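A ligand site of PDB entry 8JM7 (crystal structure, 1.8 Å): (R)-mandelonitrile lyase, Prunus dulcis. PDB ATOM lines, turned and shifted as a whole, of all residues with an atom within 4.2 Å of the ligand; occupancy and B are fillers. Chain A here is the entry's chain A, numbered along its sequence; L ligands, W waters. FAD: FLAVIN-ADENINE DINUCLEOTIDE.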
ATOM      1  N   ILE A  40      19.777  31.561 -15.540  1.00  0.00           N
ATOM      2  CA  ILE A  40      20.357  32.370 -14.425  1.00  0.00           C
ATOM      3  C   ILE A  40      19.927  31.712 -13.120  1.00  0.00           C
ATOM      4  O   ILE A  40      18.713  31.744 -12.814  1.00  0.00           O
ATOM      5  CB  ILE A  40      19.869  33.826 -14.491  1.00  0.00           C
ATOM      6  CG1 ILE A  40      20.238  34.487 -15.821  1.00  0.00           C
ATOM      7  CG2 ILE A  40      20.391  34.596 -13.316  1.00  0.00           C
ATOM      8  CD1 ILE A  40      19.371  35.605 -16.216  1.00  0.00           C
ATOM      9  N   GLY A  41      20.887  31.109 -12.457  1.00  0.00           N
ATOM     10  CA  GLY A  41      20.657  30.433 -11.157  1.00  0.00           C
ATOM     11  C   GLY A  41      20.658  28.930 -11.302  1.00  0.00           C
ATOM     12  O   GLY A  41      19.691  28.394 -11.907  1.00  0.00           O
ATOM     13  N   GLY A  42      21.697  28.285 -10.793  1.00  0.00           N
ATOM     14  CA  GLY A  42      21.854  26.817 -10.877  1.00  0.00           C
ATOM     15  C   GLY A  42      21.188  26.171  -9.685  1.00  0.00           C
ATOM     16  O   GLY A  42      21.872  25.512  -8.893  1.00  0.00           O
ATOM     17  N   GLY A  43      19.905  26.396  -9.526  1.00  0.00           N
ATOM     18  CA  GLY A  43      19.207  25.906  -8.334  1.00  0.00           C
ATOM     19  C   GLY A  43      18.247  24.793  -8.637  1.00  0.00           C
ATOM     20  O   GLY A  43      18.429  24.030  -9.628  1.00  0.00           O
ATOM     21  N   THR A  44      17.209  24.721  -7.803  1.00  0.00           N
ATOM     22  CA  THR A  44      16.198  23.649  -7.814  1.00  0.00           C
ATOM     23  C   THR A  44      15.587  23.497  -9.193  1.00  0.00           C
ATOM     24  O   THR A  44      15.564  22.374  -9.751  1.00  0.00           O
ATOM     25  CB  THR A  44      15.165  23.941  -6.706  1.00  0.00           C
ATOM     26  OG1 THR A  44      15.891  24.170  -5.490  1.00  0.00           O
ATOM     27  CG2 THR A  44      14.199  22.797  -6.577  1.00  0.00           C
ATOM     28  N   SER A  45      15.059  24.582  -9.765  1.00  0.00           N
ATOM     29  CA  SER A  45      14.487  24.577 -11.126  1.00  0.00           C
ATOM     30  C   SER A  45      15.597  24.727 -12.178  1.00  0.00           C
ATOM     31  O   SER A  45      15.471  24.142 -13.271  1.00  0.00           O
ATOM     32  CB  SER A  45      13.429  25.644 -11.319  1.00  0.00           C
ATOM     33  OG  SER A  45      12.305  25.442 -10.471  1.00  0.00           O
ATOM     34  N   LEU A  62      24.494  29.962 -15.249  1.00  0.00           N
ATOM     35  CA  LEU A  62      25.294  30.912 -14.445  1.00  0.00           C
ATOM     36  C   LEU A  62      24.819  30.782 -13.014  1.00  0.00           C
ATOM     37  O   LEU A  62      23.631  31.017 -12.789  1.00  0.00           O
ATOM     38  CB  LEU A  62      25.065  32.314 -15.001  1.00  0.00           C
ATOM     39  CG  LEU A  62      25.554  32.536 -16.441  1.00  0.00           C
ATOM     40  CD1 LEU A  62      25.153  33.890 -16.986  1.00  0.00           C
ATOM     41  CD2 LEU A  62      27.067  32.349 -16.466  1.00  0.00           C
ATOM     42  N   GLU A  63      25.714  30.404 -12.129  1.00  0.00           N
ATOM     43  CA  GLU A  63      25.412  30.306 -10.694  1.00  0.00           C
ATOM     44  C   GLU A  63      26.341  31.228  -9.905  1.00  0.00           C
ATOM     45  O   GLU A  63      27.580  31.098 -10.027  1.00  0.00           O
ATOM     46  CB  GLU A  63      25.531  28.860 -10.266  1.00  0.00           C
ATOM     47  CG  GLU A  63      25.518  28.656  -8.769  1.00  0.00           C
ATOM     48  CD  GLU A  63      24.296  29.181  -8.020  1.00  0.00           C
ATOM     49  OE1 GLU A  63      23.155  29.080  -8.561  1.00  0.00           O
ATOM     50  OE2 GLU A  63      24.492  29.756  -6.910  1.00  0.00           O
ATOM     51  N   ARG A  64      25.775  32.004  -8.970  1.00  0.00           N
ATOM     52  CA  ARG A  64      26.595  32.925  -8.154  1.00  0.00           C
ATOM     53  C   ARG A  64      27.458  32.188  -7.130  1.00  0.00           C
ATOM     54  O   ARG A  64      28.524  32.731  -6.730  1.00  0.00           O
ATOM     55  CB  ARG A  64      25.697  33.970  -7.485  1.00  0.00           C
ATOM     56  CG  ARG A  64      24.753  33.386  -6.454  1.00  0.00           C
ATOM     57  CD  ARG A  64      23.907  34.457  -5.788  1.00  0.00           C
ATOM     58  NE  ARG A  64      23.102  33.824  -4.737  1.00  0.00           N
ATOM     59  CZ  ARG A  64      22.759  34.405  -3.588  1.00  0.00           C
ATOM     60  NH1 ARG A  64      23.110  35.643  -3.355  1.00  0.00           N
ATOM     61  NH2 ARG A  64      22.165  33.689  -2.648  1.00  0.00           N
ATOM     62  N   VAL A 106      16.999  32.090   5.631  1.00  0.00           N
ATOM     63  CA  VAL A 106      18.197  31.736   4.826  1.00  0.00           C
ATOM     64  C   VAL A 106      17.764  31.390   3.409  1.00  0.00           C
ATOM     65  O   VAL A 106      16.585  30.990   3.163  1.00  0.00           O
ATOM     66  CB  VAL A 106      19.011  30.558   5.417  1.00  0.00           C
ATOM     67  CG1 VAL A 106      19.518  30.801   6.816  1.00  0.00           C
ATOM     68  CG2 VAL A 106      18.237  29.267   5.358  1.00  0.00           C
ATOM     69  N   ALA A 108      19.900  29.745  -0.383  1.00  0.00           N
ATOM     70  CA  ALA A 108      21.121  29.039  -0.818  1.00  0.00           C
ATOM     71  C   ALA A 108      21.978  29.933  -1.725  1.00  0.00           C
ATOM     72  O   ALA A 108      21.422  30.813  -2.428  1.00  0.00           O
ATOM     73  CB  ALA A 108      20.802  27.732  -1.470  1.00  0.00           C
ATOM     74  N   ARG A 109      23.266  29.639  -1.743  1.00  0.00           N
ATOM     75  CA  ARG A 109      24.266  30.328  -2.586  1.00  0.00           C
ATOM     76  C   ARG A 109      25.299  29.271  -2.987  1.00  0.00           C
ATOM     77  O   ARG A 109      26.349  29.257  -2.348  1.00  0.00           O
ATOM     78  CB  ARG A 109      24.906  31.485  -1.789  1.00  0.00           C
ATOM     79  CG  ARG A 109      25.867  32.339  -2.596  1.00  0.00           C
ATOM     80  CD  ARG A 109      26.269  33.642  -1.892  1.00  0.00           C
ATOM     81  NE  ARG A 109      26.642  33.324  -0.566  1.00  0.00           N
ATOM     82  CZ  ARG A 109      26.543  34.020   0.540  1.00  0.00           C
ATOM     83  NH1 ARG A 109      26.015  35.218   0.698  1.00  0.00           N
ATOM     84  NH2 ARG A 109      26.912  33.374   1.599  1.00  0.00           N
ATOM     85  N   ILE A 110      24.926  28.375  -3.908  1.00  0.00           N
ATOM     86  CA  ILE A 110      25.707  27.148  -4.194  1.00  0.00           C
ATOM     87  C   ILE A 110      25.099  26.524  -5.436  1.00  0.00           C
ATOM     88  O   ILE A 110      23.889  26.656  -5.648  1.00  0.00           O
ATOM     89  CB  ILE A 110      25.698  26.191  -2.961  1.00  0.00           C
ATOM     90  CG1 ILE A 110      26.880  25.222  -2.968  1.00  0.00           C
ATOM     91  CG2 ILE A 110      24.362  25.498  -2.877  1.00  0.00           C
ATOM     92  CD1 ILE A 110      28.224  25.925  -2.748  1.00  0.00           C
ATOM     93  N   GLY A 113      21.583  24.972  -5.635  1.00  0.00           N
ATOM     94  CA  GLY A 113      20.637  25.844  -4.940  1.00  0.00           C
ATOM     95  C   GLY A 113      20.172  25.265  -3.626  1.00  0.00           C
ATOM     96  O   GLY A 113      20.968  24.664  -2.862  1.00  0.00           O
ATOM     97  N   THR A 114      18.896  25.470  -3.347  1.00  0.00           N
ATOM     98  CA  THR A 114      18.369  25.193  -1.989  1.00  0.00           C
ATOM     99  C   THR A 114      18.281  23.677  -1.768  1.00  0.00           C
ATOM    100  O   THR A 114      18.388  23.273  -0.595  1.00  0.00           O
ATOM    101  CB  THR A 114      17.114  26.048  -1.757  1.00  0.00           C
ATOM    102  OG1 THR A 114      17.572  27.389  -1.843  1.00  0.00           O
ATOM    103  CG2 THR A 114      16.554  25.843  -0.356  1.00  0.00           C
ATOM    104  N   ILE A 117      21.083  22.527   0.688  1.00  0.00           N
ATOM    105  CA  ILE A 117      21.068  22.939   2.117  1.00  0.00           C
ATOM    106  C   ILE A 117      19.774  22.533   2.820  1.00  0.00           C
ATOM    107  O   ILE A 117      19.642  22.891   4.001  1.00  0.00           O
ATOM    108  CB  ILE A 117      21.339  24.435   2.296  1.00  0.00           C
ATOM    109  CG1 ILE A 117      20.222  25.259   1.655  1.00  0.00           C
ATOM    110  CG2 ILE A 117      22.734  24.844   1.750  1.00  0.00           C
ATOM    111  CD1 ILE A 117      20.199  26.752   2.114  1.00  0.00           C
ATOM    112  N   ASN A 118      18.827  21.889   2.137  1.00  0.00           N
ATOM    113  CA  ASN A 118      17.470  21.796   2.685  1.00  0.00           C
ATOM    114  C   ASN A 118      17.315  20.560   3.574  1.00  0.00           C
ATOM    115  O   ASN A 118      18.269  19.761   3.792  1.00  0.00           O
ATOM    116  CB  ASN A 118      16.400  21.934   1.607  1.00  0.00           C
ATOM    117  CG  ASN A 118      16.313  20.803   0.636  1.00  0.00           C
ATOM    118  OD1 ASN A 118      16.860  19.721   0.859  1.00  0.00           O
ATOM    119  ND2 ASN A 118      15.540  21.010  -0.404  1.00  0.00           N
ATOM    120  N   ALA A 119      16.072  20.304   3.990  1.00  0.00           N
ATOM    121  CA  ALA A 119      15.819  19.201   4.940  1.00  0.00           C
ATOM    122  C   ALA A 119      15.456  17.896   4.220  1.00  0.00           C
ATOM    123  O   ALA A 119      15.135  16.943   4.925  1.00  0.00           O
ATOM    124  CB  ALA A 119      14.754  19.621   5.907  1.00  0.00           C
ATOM    125  N   GLY A 120      15.565  17.841   2.889  1.00  0.00           N
ATOM    126  CA  GLY A 120      15.480  16.647   2.024  1.00  0.00           C
ATOM    127  C   GLY A 120      14.092  16.067   1.799  1.00  0.00           C
ATOM    128  O   GLY A 120      13.967  15.012   1.155  1.00  0.00           O
ATOM    129  N   VAL A 121      13.043  16.659   2.360  1.00  0.00           N
ATOM    130  CA  VAL A 121      11.708  16.013   2.252  1.00  0.00           C
ATOM    131  C   VAL A 121      11.266  16.121   0.790  1.00  0.00           C
ATOM    132  O   VAL A 121      11.302  17.232   0.213  1.00  0.00           O
ATOM    133  CB  VAL A 121      10.697  16.679   3.221  1.00  0.00           C
ATOM    134  CG1 VAL A 121       9.341  15.985   3.136  1.00  0.00           C
ATOM    135  CG2 VAL A 121      11.272  16.698   4.611  1.00  0.00           C
ATOM    136  N   ALA A 223      29.486  33.122 -10.671  1.00  0.00           N
ATOM    137  CA  ALA A 223      29.000  34.022 -11.733  1.00  0.00           C
ATOM    138  C   ALA A 223      27.809  34.778 -11.193  1.00  0.00           C
ATOM    139  O   ALA A 223      26.680  34.208 -11.101  1.00  0.00           O
ATOM    140  CB  ALA A 223      28.606  33.287 -13.001  1.00  0.00           C
ATOM    141  N   SER A 224      28.028  36.044 -10.832  1.00  0.00           N
ATOM    142  CA  SER A 224      26.974  36.878 -10.230  1.00  0.00           C
ATOM    143  C   SER A 224      26.320  37.687 -11.351  1.00  0.00           C
ATOM    144  O   SER A 224      26.970  38.632 -11.899  1.00  0.00           O
ATOM    145  CB  SER A 224      27.548  37.653  -9.022  1.00  0.00           C
ATOM    146  OG  SER A 224      26.850  38.839  -8.833  1.00  0.00           O
ATOM    147  N   VAL A 225      25.110  37.287 -11.765  1.00  0.00           N
ATOM    148  CA  VAL A 225      24.375  37.916 -12.895  1.00  0.00           C
ATOM    149  C   VAL A 225      23.763  39.228 -12.386  1.00  0.00           C
ATOM    150  O   VAL A 225      22.985  39.173 -11.412  1.00  0.00           O
ATOM    151  CB  VAL A 225      23.298  37.004 -13.491  1.00  0.00           C
ATOM    152  CG1 VAL A 225      22.510  37.701 -14.554  1.00  0.00           C
ATOM    153  CG2 VAL A 225      23.910  35.755 -14.064  1.00  0.00           C
ATOM    154  N   SER A 265      15.993  31.807 -13.072  1.00  0.00           N
ATOM    155  CA  SER A 265      15.791  30.709 -12.103  1.00  0.00           C
ATOM    156  C   SER A 265      16.528  31.051 -10.803  1.00  0.00           C
ATOM    157  O   SER A 265      17.057  30.158 -10.198  1.00  0.00           O
ATOM    158  CB  SER A 265      16.245  29.390 -12.730  1.00  0.00           C
ATOM    159  OG  SER A 265      15.431  29.096 -13.855  1.00  0.00           O
ATOM    160  N   ALA A 266      16.538  32.336 -10.437  1.00  0.00           N
ATOM    161  CA  ALA A 266      17.374  32.862  -9.321  1.00  0.00           C
ATOM    162  C   ALA A 266      16.607  32.810  -7.979  1.00  0.00           C
ATOM    163  O   ALA A 266      17.098  33.389  -6.992  1.00  0.00           O
ATOM    164  CB  ALA A 266      17.828  34.251  -9.684  1.00  0.00           C
ATOM    165  N   GLY A 267      15.395  32.279  -7.989  1.00  0.00           N
ATOM    166  CA  GLY A 267      14.623  32.049  -6.751  1.00  0.00           C
ATOM    167  C   GLY A 267      13.660  33.194  -6.419  1.00  0.00           C
ATOM    168  O   GLY A 267      13.649  34.257  -7.056  1.00  0.00           O
ATOM    169  N   GLY A 270      16.027  36.128  -5.680  1.00  0.00           N
ATOM    170  CA  GLY A 270      16.940  36.565  -6.757  1.00  0.00           C
ATOM    171  C   GLY A 270      16.236  36.993  -8.029  1.00  0.00           C
ATOM    172  O   GLY A 270      16.751  37.879  -8.774  1.00  0.00           O
ATOM    173  N   VAL A 388      24.051  43.555  -7.333  1.00  0.00           N
ATOM    174  CA  VAL A 388      23.196  42.349  -7.125  1.00  0.00           C
ATOM    175  C   VAL A 388      23.671  41.600  -5.887  1.00  0.00           C
ATOM    176  O   VAL A 388      22.886  40.790  -5.360  1.00  0.00           O
ATOM    177  CB  VAL A 388      23.186  41.438  -8.344  1.00  0.00           C
ATOM    178  CG1 VAL A 388      24.478  40.617  -8.485  1.00  0.00           C
ATOM    179  CG2 VAL A 388      21.956  40.561  -8.328  1.00  0.00           C
ATOM    180  N   TRP A 467      10.631  28.269   5.547  1.00  0.00           N
ATOM    181  CA  TRP A 467      11.686  28.323   4.499  1.00  0.00           C
ATOM    182  C   TRP A 467      11.107  28.035   3.111  1.00  0.00           C
ATOM    183  O   TRP A 467      11.901  27.814   2.145  1.00  0.00           O
ATOM    184  CB  TRP A 467      12.823  27.338   4.771  1.00  0.00           C
ATOM    185  CG  TRP A 467      13.510  27.492   6.082  1.00  0.00           C
ATOM    186  CD1 TRP A 467      14.138  28.604   6.541  1.00  0.00           C
ATOM    187  CD2 TRP A 467      13.850  26.450   7.005  1.00  0.00           C
ATOM    188  NE1 TRP A 467      14.766  28.342   7.738  1.00  0.00           N
ATOM    189  CE2 TRP A 467      14.557  27.053   8.071  1.00  0.00           C
ATOM    190  CE3 TRP A 467      13.531  25.086   7.097  1.00  0.00           C
ATOM    191  CZ2 TRP A 467      15.071  26.307   9.143  1.00  0.00           C
ATOM    192  CZ3 TRP A 467      14.037  24.362   8.162  1.00  0.00           C
ATOM    193  CH2 TRP A 467      14.762  24.972   9.192  1.00  0.00           C
ATOM    194  N   HIS A 468       9.800  27.919   2.991  1.00  0.00           N
ATOM    195  CA  HIS A 468       9.163  27.536   1.721  1.00  0.00           C
ATOM    196  C   HIS A 468       8.557  28.766   1.055  1.00  0.00           C
ATOM    197  O   HIS A 468       7.467  28.683   0.503  1.00  0.00           O
ATOM    198  CB  HIS A 468       8.134  26.446   1.946  1.00  0.00           C
ATOM    199  CG  HIS A 468       8.670  25.184   2.482  1.00  0.00           C
ATOM    200  ND1 HIS A 468       7.818  24.134   2.760  1.00  0.00           N
ATOM    201  CD2 HIS A 468       9.912  24.767   2.822  1.00  0.00           C
ATOM    202  CE1 HIS A 468       8.562  23.122   3.190  1.00  0.00           C
ATOM    203  NE2 HIS A 468       9.800  23.489   3.277  1.00  0.00           N
ATOM    204  N   ASP A 495      11.111  29.037 -11.360  1.00  0.00           N
ATOM    205  CA  ASP A 495      11.601  28.806  -9.978  1.00  0.00           C
ATOM    206  C   ASP A 495      10.405  29.041  -9.038  1.00  0.00           C
ATOM    207  O   ASP A 495       9.252  29.225  -9.537  1.00  0.00           O
ATOM    208  CB  ASP A 495      12.800  29.694  -9.673  1.00  0.00           C
ATOM    209  CG  ASP A 495      12.522  31.188  -9.787  1.00  0.00           C
ATOM    210  OD1 ASP A 495      11.349  31.576  -9.791  1.00  0.00           O
ATOM    211  OD2 ASP A 495      13.517  31.955  -9.936  1.00  0.00           O
ATOM    212  N   ALA A 496      10.639  29.183  -7.749  1.00  0.00           N
ATOM    213  CA  ALA A 496       9.552  29.343  -6.758  1.00  0.00           C
ATOM    214  C   ALA A 496       8.996  30.767  -6.770  1.00  0.00           C
ATOM    215  O   ALA A 496       8.015  30.989  -6.069  1.00  0.00           O
ATOM    216  CB  ALA A 496      10.003  28.936  -5.379  1.00  0.00           C
ATOM    217  N   HIS A 506       5.923  20.477   0.984  1.00  0.00           N
ATOM    218  CA  HIS A 506       7.379  20.398   0.743  1.00  0.00           C
ATOM    219  C   HIS A 506       7.589  20.528  -0.758  1.00  0.00           C
ATOM    220  O   HIS A 506       7.415  19.574  -1.485  1.00  0.00           O
ATOM    221  CB  HIS A 506       7.937  19.100   1.342  1.00  0.00           C
ATOM    222  CG  HIS A 506       7.924  19.108   2.823  1.00  0.00           C
ATOM    223  ND1 HIS A 506       6.822  18.720   3.529  1.00  0.00           N
ATOM    224  CD2 HIS A 506       8.823  19.544   3.723  1.00  0.00           C
ATOM    225  CE1 HIS A 506       7.085  18.847   4.816  1.00  0.00           C
ATOM    226  NE2 HIS A 506       8.246  19.389   4.963  1.00  0.00           N
ATOM    227  N   PRO A 507       7.845  21.741  -1.249  1.00  0.00           N
ATOM    228  CA  PRO A 507       7.787  22.020  -2.671  1.00  0.00           C
ATOM    229  C   PRO A 507       9.002  21.700  -3.542  1.00  0.00           C
ATOM    230  O   PRO A 507       8.883  21.900  -4.719  1.00  0.00           O
ATOM    231  CB  PRO A 507       7.531  23.564  -2.624  1.00  0.00           C
ATOM    232  CG  PRO A 507       8.346  24.035  -1.479  1.00  0.00           C
ATOM    233  CD  PRO A 507       8.049  22.957  -0.434  1.00  0.00           C
ATOM    234  N   GLN A 508      10.113  21.236  -2.995  1.00  0.00           N
ATOM    235  CA  GLN A 508      11.325  21.000  -3.837  1.00  0.00           C
ATOM    236  C   GLN A 508      10.975  20.037  -4.979  1.00  0.00           C
ATOM    237  O   GLN A 508      11.395  20.294  -6.089  1.00  0.00           O
ATOM    238  CB  GLN A 508      12.521  20.506  -3.012  1.00  0.00           C
ATOM    239  CG  GLN A 508      12.510  19.060  -2.556  1.00  0.00           C
ATOM    240  CD  GLN A 508      13.883  18.574  -2.145  1.00  0.00           C
ATOM    241  OE1 GLN A 508      14.911  19.124  -2.564  1.00  0.00           O
ATOM    242  NE2 GLN A 508      13.949  17.552  -1.299  1.00  0.00           N
HETATM  243  PA  FAD L   1      17.053  27.990  -5.401  1.00  0.00           P
HETATM  244  O1A FAD L   1      17.117  26.486  -5.338  1.00  0.00           O
HETATM  245  O2A FAD L   1      17.427  28.775  -4.196  1.00  0.00           O
HETATM  246  O5B FAD L   1      17.854  28.437  -6.691  1.00  0.00           O
HETATM  247  C5B FAD L   1      18.199  29.797  -7.011  1.00  0.00           C
HETATM  248  C4B FAD L   1      19.665  29.857  -7.382  1.00  0.00           C
HETATM  249  O4B FAD L   1      19.941  31.175  -7.981  1.00  0.00           O
HETATM  250  C3B FAD L   1      20.629  29.698  -6.199  1.00  0.00           C
HETATM  251  O3B FAD L   1      21.489  28.581  -6.419  1.00  0.00           O
HETATM  252  C2B FAD L   1      21.291  31.080  -6.091  1.00  0.00           C
HETATM  253  O2B FAD L   1      22.591  30.981  -5.552  1.00  0.00           O
HETATM  254  C1B FAD L   1      21.241  31.557  -7.544  1.00  0.00           C
HETATM  255  N9A FAD L   1      21.294  32.968  -7.755  1.00  0.00           N
HETATM  256  C8A FAD L   1      20.459  33.946  -7.139  1.00  0.00           C
HETATM  257  N7A FAD L   1      20.641  35.128  -7.675  1.00  0.00           N
HETATM  258  C5A FAD L   1      21.595  34.919  -8.672  1.00  0.00           C
HETATM  259  C6A FAD L   1      22.203  35.827  -9.564  1.00  0.00           C
HETATM  260  N6A FAD L   1      21.888  37.117  -9.611  1.00  0.00           N
HETATM  261  N1A FAD L   1      23.118  35.323 -10.430  1.00  0.00           N
HETATM  262  C2A FAD L   1      23.425  34.019 -10.340  1.00  0.00           C
HETATM  263  N3A FAD L   1      22.898  33.057  -9.558  1.00  0.00           N
HETATM  264  C4A FAD L   1      22.003  33.615  -8.723  1.00  0.00           C
HETATM  265  N1  FAD L   1      11.486  22.097   0.466  1.00  0.00           N
HETATM  266  C2  FAD L   1      11.221  20.758   0.413  1.00  0.00           C
HETATM  267  O2  FAD L   1      10.407  20.297  -0.385  1.00  0.00           O
HETATM  268  N3  FAD L   1      11.694  19.914   1.376  1.00  0.00           N
HETATM  269  C4  FAD L   1      12.433  20.346   2.455  1.00  0.00           C
HETATM  270  O4  FAD L   1      12.905  19.508   3.227  1.00  0.00           O
HETATM  271  C4X FAD L   1      12.867  21.697   2.463  1.00  0.00           C
HETATM  272  N5  FAD L   1      13.659  22.118   3.447  1.00  0.00           N
HETATM  273  C5X FAD L   1      14.132  23.395   3.325  1.00  0.00           C
HETATM  274  C6  FAD L   1      15.094  23.849   4.257  1.00  0.00           C
HETATM  275  C7  FAD L   1      15.675  25.078   4.157  1.00  0.00           C
HETATM  276  C7M FAD L   1      16.739  25.499   5.140  1.00  0.00           C
HETATM  277  C8  FAD L   1      15.287  25.931   3.091  1.00  0.00           C
HETATM  278  C8M FAD L   1      15.930  27.283   2.916  1.00  0.00           C
HETATM  279  C9  FAD L   1      14.272  25.537   2.233  1.00  0.00           C
HETATM  280  C9A FAD L   1      13.706  24.264   2.289  1.00  0.00           C
HETATM  281  N10 FAD L   1      12.754  23.802   1.364  1.00  0.00           N
HETATM  282  C10 FAD L   1      12.327  22.522   1.398  1.00  0.00           C
HETATM  283  C1' FAD L   1      12.256  24.675   0.290  1.00  0.00           C
HETATM  284  C2' FAD L   1      12.809  24.342  -1.080  1.00  0.00           C
HETATM  285  O2' FAD L   1      14.090  23.702  -0.903  1.00  0.00           O
HETATM  286  C3' FAD L   1      12.840  25.642  -1.905  1.00  0.00           C
HETATM  287  O3' FAD L   1      11.532  26.320  -1.917  1.00  0.00           O
HETATM  288  C4' FAD L   1      13.235  25.450  -3.372  1.00  0.00           C
HETATM  289  O4' FAD L   1      14.449  24.685  -3.361  1.00  0.00           O
HETATM  290  C5' FAD L   1      13.445  26.770  -4.081  1.00  0.00           C
HETATM  291  O5' FAD L   1      13.933  26.512  -5.433  1.00  0.00           O
HETATM  292  P   FAD L   1      14.351  27.733  -6.422  1.00  0.00           P
HETATM  293  O1P FAD L   1      14.835  27.100  -7.679  1.00  0.00           O
HETATM  294  O2P FAD L   1      13.176  28.687  -6.458  1.00  0.00           O
HETATM  295  O3P FAD L   1      15.557  28.421  -5.655  1.00  0.00           O
HETATM  296  O   HOH W   1       8.828  27.316  -2.224  1.00  0.00           O
HETATM  297  O   HOH W   2      18.860  31.059  -3.404  1.00  0.00           O
HETATM  298  O   HOH W   3      16.779  27.465  -9.745  1.00  0.00           O
HETATM  299  O   HOH W   4       9.453  18.008  -2.070  1.00  0.00           O
HETATM  300  O   HOH W   5      19.434  38.419  -8.511  1.00  0.00           O
HETATM  301  O   HOH W   6      15.477  30.357  -2.965  1.00  0.00           O
HETATM  302  O   HOH W   7      11.292  22.101   5.507  1.00  0.00           O
HETATM  303  O   HOH W   8      18.207  33.405  -4.515  1.00  0.00           O
HETATM  304  O   HOH W   9      13.089  30.294  -4.119  1.00  0.00           O
HETATM  305  O   HOH W  10      11.811  29.060  -1.875  1.00  0.00           O
HETATM  306  O   HOH W  11      20.469  37.288  -5.746  1.00  0.00           O
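N of Thr 44 sits at hydrogen-bond distance from O1A of the ligand, 3.0 Å away.
OG1 of Thr 44 sits at hydrogen-bond distance from O4' of the ligand.
OE2 of Glu 63 lies within hydrogen-bond range of O2B of the ligand (2.6 Å).
N of Thr 114 sits at hydrogen-bond distance from O1A of the ligand, 2.9 Å away.
O2A of the ligand is in hydrogen-bond range of OG1 of Thr 114, 2.7 Å away.
An oxygen (O2) of the ligand lies within hydrogen-bond range of the backbone NH (N) of Gln 508.
N of Ala 496 sits at hydrogen-bond distance from O2P of the ligand (2.9 Å).
N of Val 225 lies within hydrogen-bond range of N1A of the ligand.
N6A of the ligand sits at hydrogen-bond distance from O of Val 225 (2.9 Å).
O4 of the ligand sits at hydrogen-bond distance from N of Val 121 (3.0 Å).
O of Val 121 sits at hydrogen-bond distance from N3 of the ligand, 2.9 Å away.
The backbone NH (N) of Arg 64 sits at hydrogen-bond distance from a nitrogen (N3A) of the ligand (3.1 Å).
An oxygen (O2B) of the ligand is in hydrogen-bond range of the guanidinium group of Arg 64 (3.0 Å).
A nitrogen (N5) of the ligand is in hydrogen-bond range of the backbone NH (N) of Ala 119 (3.1 Å).
An oxygen (O2') of the ligand sits at hydrogen-bond distance from the side-chain amide nitrogen of Asn 118, at 3.1 Å.
The backbone NH (N) of Gly 120 lies within hydrogen-bond range of an oxygen (O4) of the ligand.
O3B of the ligand sits at hydrogen-bond distance from O of Ile 110 (3.2 Å).
O1P of the ligand is in hydrogen-bond range of N of Ser 45 (3.3 Å).
O of Ala 108 lies within hydrogen-bond range of O2B of the ligand (3.3 Å).
OE2 of Glu 63 sits at hydrogen-bond distance from N of Ile 110 (3.3 Å).
The backbone carbonyl oxygen (O) of Glu 63 sits at hydrogen-bond distance from the backbone NH (N) of Ala 223 (2.9 Å).
NE2 of Gln 508 sits at hydrogen-bond distance from O of Val 121 (3.1 Å).
The side-chain amide oxygen (OD1) of Asn 118 sits at hydrogen-bond distance from the backbone NH (N) of Gly 120 (3.1 Å).
The backbone NH of Gly 41 sits at hydrogen-bond distance from the backbone carbonyl oxygen of Leu 62 (2.8 Å).
N of Ala 266 lies within hydrogen-bond range of OD2 of Asp 495 (3.1 Å).
The backbone carbonyl oxygen (O) of Ile 40 is in hydrogen-bond range of the backbone NH (N) of Ala 266 (3.3 Å).
The backbone NH (N) of Gly 267 lies within hydrogen-bond range of the side-chain carboxylate (OD2) of Asp 495 (2.7 Å).
The backbone carbonyl oxygen (O) of His 506 sits close to an oxygen (O2) of the ligand (3.3 Å).
The backbone nitrogen (N) of Pro 507 sits close to an oxygen (O2) of the ligand, 3.1 Å away.
Gly 41 touches the ligand.
Gly 42 touches the ligand.
Gly 43 touches the ligand.
Leu 62 touches the ligand (O to C2A, 3.9 Å).
Val 106 touches the ligand (O to C8M, 3.8 Å).
Arg 109 touches the ligand (CA to O2B, 3.5 Å).
Gly 113 touches the ligand (CA to O3B, 3.2 Å).
Ala 223 touches the ligand.
O of Ser 265 touches C5B of the ligand (3.4 Å).
Ala 266 touches the ligand.
CA of Gly 267 touches O2P of the ligand (3.7 Å).
Val 388 touches the ligand.
Trp 467 touches the ligand (O to C9, 3.3 Å).
His 468 touches the ligand (NE2 to C10, 3.3 Å).
Asp 495 touches the ligand.
Of the 35 residues printed, 31 come within 4 Å of the ligand.
Water W2 bridges the backbone carbonyl oxygen (O) of Ala 108 and an oxygen (O2A) of the ligand.
Water W1 lies within hydrogen-bond range of O3' of the ligand (2.9 Å) and O of His 468 (3.3 Å).
Water W5 lies within hydrogen-bond range of O of Gly 270 and N6A of the ligand.
Water W7 bridges NE2 of His 468 and N5 of the ligand.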
